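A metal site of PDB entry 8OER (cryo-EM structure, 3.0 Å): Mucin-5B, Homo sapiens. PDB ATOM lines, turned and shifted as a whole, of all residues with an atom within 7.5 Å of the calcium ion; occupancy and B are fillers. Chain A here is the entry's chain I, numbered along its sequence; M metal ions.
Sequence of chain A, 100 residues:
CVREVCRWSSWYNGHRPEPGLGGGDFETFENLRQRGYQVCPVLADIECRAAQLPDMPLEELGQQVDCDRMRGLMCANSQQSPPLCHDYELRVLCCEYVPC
The side-chain carboxylate (OE1) of Glu 27 is in hydrogen-bond range of the backbone NH (N) of Gly 14 (3.4 Å).
O of Glu 27 is in hydrogen-bond range of N of Leu 73 (2.9 Å).
The backbone carbonyl oxygen (O) of Gly 24 lies within hydrogen-bond range of a ring nitrogen (NE2) of His 15, at 3.0 Å.
The calcium ion is bound by the side-chain carboxylate of Glu 27 (2.3 Å), the side-chain carboxylate of Asp 25 (2.3 Å), the side-chain amide oxygen of Asn 13 (2.4 Å), the backbone carbonyl oxygen of His 15 (2.5 Å) and the backbone carbonyl oxygen of Tyr 88 (2.8 Å).
Slightly farther from the calcium ion lies the side-chain carboxylate (OD1) of Asp 25 (3.0 Å).
Of the 17 residues printed, 5 come within 4 Å of the calcium ion.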
ATOM      1  N   TYR A  12     -25.024   8.143  -4.640  1.00  0.00           N
ATOM      2  CA  TYR A  12     -25.318   9.579  -4.601  1.00  0.00           C
ATOM      3  C   TYR A  12     -24.070  10.354  -4.996  1.00  0.00           C
ATOM      4  O   TYR A  12     -23.157  10.538  -4.171  1.00  0.00           O
ATOM      5  CB  TYR A  12     -25.813   9.999  -3.220  1.00  0.00           C
ATOM      6  CG  TYR A  12     -27.133   9.388  -2.825  1.00  0.00           C
ATOM      7  CD1 TYR A  12     -28.334   9.960  -3.252  1.00  0.00           C
ATOM      8  CD2 TYR A  12     -27.190   8.248  -2.035  1.00  0.00           C
ATOM      9  CE1 TYR A  12     -29.542   9.405  -2.893  1.00  0.00           C
ATOM     10  CE2 TYR A  12     -28.397   7.693  -1.675  1.00  0.00           C
ATOM     11  CZ  TYR A  12     -29.575   8.267  -2.110  1.00  0.00           C
ATOM     12  OH  TYR A  12     -30.783   7.713  -1.751  1.00  0.00           O
ATOM     13  N   ASN A  13     -24.011  10.821  -6.243  1.00  0.00           N
ATOM     14  CA  ASN A  13     -22.915  11.651  -6.734  1.00  0.00           C
ATOM     15  C   ASN A  13     -23.490  13.020  -7.071  1.00  0.00           C
ATOM     16  O   ASN A  13     -23.840  13.308  -8.211  1.00  0.00           O
ATOM     17  CB  ASN A  13     -22.255  11.005  -7.953  1.00  0.00           C
ATOM     18  CG  ASN A  13     -21.000  11.741  -8.391  1.00  0.00           C
ATOM     19  OD1 ASN A  13     -20.611  12.740  -7.794  1.00  0.00           O
ATOM     20  ND2 ASN A  13     -20.359  11.234  -9.440  1.00  0.00           N
ATOM     21  N   GLY A  14     -23.561  13.887  -6.055  1.00  0.00           N
ATOM     22  CA  GLY A  14     -24.174  15.194  -6.180  1.00  0.00           C
ATOM     23  C   GLY A  14     -23.244  16.329  -6.542  1.00  0.00           C
ATOM     24  O   GLY A  14     -23.676  17.489  -6.537  1.00  0.00           O
ATOM     25  N   HIS A  15     -21.986  16.048  -6.854  1.00  0.00           N
ATOM     26  CA  HIS A  15     -21.021  17.099  -7.134  1.00  0.00           C
ATOM     27  C   HIS A  15     -19.910  16.533  -8.009  1.00  0.00           C
ATOM     28  O   HIS A  15     -19.651  15.321  -8.004  1.00  0.00           O
ATOM     29  CB  HIS A  15     -20.440  17.674  -5.838  1.00  0.00           C
ATOM     30  CG  HIS A  15     -19.373  18.703  -6.047  1.00  0.00           C
ATOM     31  ND1 HIS A  15     -19.641  20.013  -6.331  1.00  0.00           N
ATOM     32  CD2 HIS A  15     -18.024  18.593  -6.008  1.00  0.00           C
ATOM     33  CE1 HIS A  15     -18.505  20.683  -6.460  1.00  0.00           C
ATOM     34  NE2 HIS A  15     -17.507  19.841  -6.265  1.00  0.00           N
ATOM     35  N   ARG A  16     -19.258  17.417  -8.751  1.00  0.00           N
ATOM     36  CA  ARG A  16     -18.079  17.057  -9.524  1.00  0.00           C
ATOM     37  C   ARG A  16     -16.911  17.887  -9.034  1.00  0.00           C
ATOM     38  O   ARG A  16     -16.934  19.114  -9.183  1.00  0.00           O
ATOM     39  CB  ARG A  16     -18.319  17.281 -11.014  1.00  0.00           C
ATOM     40  CG  ARG A  16     -19.324  16.325 -11.614  1.00  0.00           C
ATOM     41  CD  ARG A  16     -18.929  14.873 -11.354  1.00  0.00           C
ATOM     42  NE  ARG A  16     -19.562  13.913 -12.245  1.00  0.00           N
ATOM     43  CZ  ARG A  16     -19.597  13.977 -13.572  1.00  0.00           C
ATOM     44  NH1 ARG A  16     -18.950  14.922 -14.233  1.00  0.00           N
ATOM     45  NH2 ARG A  16     -20.274  13.057 -14.253  1.00  0.00           N
ATOM     46  N   PRO A  17     -15.886  17.260  -8.433  1.00  0.00           N
ATOM     47  CA  PRO A  17     -14.825  18.045  -7.805  1.00  0.00           C
ATOM     48  C   PRO A  17     -14.125  18.962  -8.793  1.00  0.00           C
ATOM     49  O   PRO A  17     -13.964  18.646  -9.976  1.00  0.00           O
ATOM     50  CB  PRO A  17     -13.869  16.972  -7.262  1.00  0.00           C
ATOM     51  CG  PRO A  17     -14.264  15.710  -7.946  1.00  0.00           C
ATOM     52  CD  PRO A  17     -15.717  15.820  -8.214  1.00  0.00           C
ATOM     53  N   GLY A  24     -12.530  20.269  -4.731  1.00  0.00           N
ATOM     54  CA  GLY A  24     -12.679  18.937  -4.208  1.00  0.00           C
ATOM     55  C   GLY A  24     -14.136  18.546  -4.173  1.00  0.00           C
ATOM     56  O   GLY A  24     -14.988  19.229  -4.730  1.00  0.00           O
ATOM     57  N   ASP A  25     -14.413  17.446  -3.496  1.00  0.00           N
ATOM     58  CA  ASP A  25     -15.772  16.932  -3.381  1.00  0.00           C
ATOM     59  C   ASP A  25     -16.226  17.044  -1.938  1.00  0.00           C
ATOM     60  O   ASP A  25     -15.506  16.634  -1.025  1.00  0.00           O
ATOM     61  CB  ASP A  25     -15.868  15.477  -3.849  1.00  0.00           C
ATOM     62  CG  ASP A  25     -17.276  15.109  -4.288  1.00  0.00           C
ATOM     63  OD1 ASP A  25     -18.157  15.988  -4.241  1.00  0.00           O
ATOM     64  OD2 ASP A  25     -17.499  13.942  -4.688  1.00  0.00           O
ATOM     65  N   PHE A  26     -17.416  17.608  -1.730  1.00  0.00           N
ATOM     66  CA  PHE A  26     -17.961  17.831  -0.388  1.00  0.00           C
ATOM     67  C   PHE A  26     -19.387  17.291  -0.385  1.00  0.00           C
ATOM     68  O   PHE A  26     -20.337  18.043  -0.591  1.00  0.00           O
ATOM     69  CB  PHE A  26     -17.894  19.312  -0.029  1.00  0.00           C
ATOM     70  CG  PHE A  26     -16.641  19.995  -0.517  1.00  0.00           C
ATOM     71  CD1 PHE A  26     -15.475  19.944   0.231  1.00  0.00           C
ATOM     72  CD2 PHE A  26     -16.631  20.699  -1.709  1.00  0.00           C
ATOM     73  CE1 PHE A  26     -14.328  20.571  -0.213  1.00  0.00           C
ATOM     74  CE2 PHE A  26     -15.483  21.327  -2.153  1.00  0.00           C
ATOM     75  CZ  PHE A  26     -14.337  21.264  -1.400  1.00  0.00           C
ATOM     76  N   GLU A  27     -19.528  15.983  -0.139  1.00  0.00           N
ATOM     77  CA  GLU A  27     -20.817  15.303  -0.182  1.00  0.00           C
ATOM     78  C   GLU A  27     -21.315  15.165   1.249  1.00  0.00           C
ATOM     79  O   GLU A  27     -20.960  14.213   1.943  1.00  0.00           O
ATOM     80  CB  GLU A  27     -20.687  13.941  -0.857  1.00  0.00           C
ATOM     81  CG  GLU A  27     -20.155  13.966  -2.284  1.00  0.00           C
ATOM     82  CD  GLU A  27     -21.144  14.533  -3.275  1.00  0.00           C
ATOM     83  OE1 GLU A  27     -22.351  14.590  -2.954  1.00  0.00           O
ATOM     84  OE2 GLU A  27     -20.723  14.883  -4.395  1.00  0.00           O
ATOM     85  N   ALA A  51     -16.369   7.303  -7.899  1.00  0.00           N
ATOM     86  CA  ALA A  51     -17.380   7.024  -8.912  1.00  0.00           C
ATOM     87  C   ALA A  51     -16.758   6.542 -10.213  1.00  0.00           C
ATOM     88  O   ALA A  51     -17.300   5.643 -10.868  1.00  0.00           O
ATOM     89  CB  ALA A  51     -18.238   8.266  -9.149  1.00  0.00           C
ATOM     90  N   LEU A  73     -18.955  12.491   3.145  1.00  0.00           N
ATOM     91  CA  LEU A  73     -17.663  12.324   2.475  1.00  0.00           C
ATOM     92  C   LEU A  73     -17.068  13.679   2.156  1.00  0.00           C
ATOM     93  O   LEU A  73     -17.775  14.597   1.724  1.00  0.00           O
ATOM     94  CB  LEU A  73     -17.835  11.480   1.205  1.00  0.00           C
ATOM     95  CG  LEU A  73     -16.733  11.091   0.221  1.00  0.00           C
ATOM     96  CD1 LEU A  73     -17.346  10.134  -0.783  1.00  0.00           C
ATOM     97  CD2 LEU A  73     -16.116  12.255  -0.534  1.00  0.00           C
ATOM     98  N   HIS A  86     -10.419  12.914  -6.748  1.00  0.00           N
ATOM     99  CA  HIS A  86     -11.201  12.152  -7.707  1.00  0.00           C
ATOM    100  C   HIS A  86     -12.680  12.474  -7.508  1.00  0.00           C
ATOM    101  O   HIS A  86     -13.060  13.201  -6.585  1.00  0.00           O
ATOM    102  CB  HIS A  86     -10.915  10.657  -7.533  1.00  0.00           C
ATOM    103  CG  HIS A  86      -9.467  10.312  -7.649  1.00  0.00           C
ATOM    104  ND1 HIS A  86      -8.814   9.531  -6.708  1.00  0.00           N
ATOM    105  CD2 HIS A  86      -8.535  10.629  -8.579  1.00  0.00           C
ATOM    106  CE1 HIS A  86      -7.555   9.385  -7.070  1.00  0.00           C
ATOM    107  NE2 HIS A  86      -7.359  10.038  -8.196  1.00  0.00           N
ATOM    108  N   ASP A  87     -13.527  11.942  -8.383  1.00  0.00           N
ATOM    109  CA  ASP A  87     -14.967  12.166  -8.281  1.00  0.00           C
ATOM    110  C   ASP A  87     -15.576  11.024  -7.481  1.00  0.00           C
ATOM    111  O   ASP A  87     -15.740   9.915  -7.990  1.00  0.00           O
ATOM    112  CB  ASP A  87     -15.594  12.272  -9.672  1.00  0.00           C
ATOM    113  CG  ASP A  87     -14.945  13.338 -10.531  1.00  0.00           C
ATOM    114  OD1 ASP A  87     -13.751  13.637 -10.312  1.00  0.00           O
ATOM    115  OD2 ASP A  87     -15.617  13.883 -11.427  1.00  0.00           O
ATOM    116  N   TYR A  88     -15.931  11.303  -6.230  1.00  0.00           N
ATOM    117  CA  TYR A  88     -16.420  10.282  -5.316  1.00  0.00           C
ATOM    118  C   TYR A  88     -17.942  10.297  -5.262  1.00  0.00           C
ATOM    119  O   TYR A  88     -18.602  11.225  -5.723  1.00  0.00           O
ATOM    120  CB  TYR A  88     -15.855  10.489  -3.901  1.00  0.00           C
ATOM    121  CG  TYR A  88     -14.353  10.427  -3.761  1.00  0.00           C
ATOM    122  CD1 TYR A  88     -13.555  11.463  -4.214  1.00  0.00           C
ATOM    123  CD2 TYR A  88     -13.739   9.348  -3.142  1.00  0.00           C
ATOM    124  CE1 TYR A  88     -12.185  11.420  -4.077  1.00  0.00           C
ATOM    125  CE2 TYR A  88     -12.365   9.292  -2.995  1.00  0.00           C
ATOM    126  CZ  TYR A  88     -11.597  10.334  -3.475  1.00  0.00           C
ATOM    127  OH  TYR A  88     -10.231  10.301  -3.335  1.00  0.00           O
ATOM    128  N   GLU A  89     -18.486   9.228  -4.671  1.00  0.00           N
ATOM    129  CA  GLU A  89     -19.892   9.189  -4.288  1.00  0.00           C
ATOM    130  C   GLU A  89     -20.019   8.223  -3.110  1.00  0.00           C
ATOM    131  O   GLU A  89     -19.042   7.613  -2.682  1.00  0.00           O
ATOM    132  CB  GLU A  89     -20.804   8.783  -5.462  1.00  0.00           C
ATOM    133  CG  GLU A  89     -21.129   7.298  -5.671  1.00  0.00           C
ATOM    134  CD  GLU A  89     -19.953   6.344  -5.574  1.00  0.00           C
ATOM    135  OE1 GLU A  89     -20.205   5.121  -5.542  1.00  0.00           O
ATOM    136  OE2 GLU A  89     -18.788   6.781  -5.606  1.00  0.00           O
ATOM    137  N   LEU A  90     -21.237   8.104  -2.581  1.00  0.00           N
ATOM    138  CA  LEU A  90     -21.460   7.318  -1.382  1.00  0.00           C
ATOM    139  C   LEU A  90     -22.897   6.812  -1.359  1.00  0.00           C
ATOM    140  O   LEU A  90     -23.754   7.291  -2.100  1.00  0.00           O
ATOM    141  CB  LEU A  90     -21.154   8.119  -0.109  1.00  0.00           C
ATOM    142  CG  LEU A  90     -21.842   9.476   0.072  1.00  0.00           C
ATOM    143  CD1 LEU A  90     -21.828   9.878   1.535  1.00  0.00           C
ATOM    144  CD2 LEU A  90     -21.149  10.536  -0.745  1.00  0.00           C
HETATM  145 CA    CA M   1     -19.406  13.879  -6.002  1.00  0.00          CA
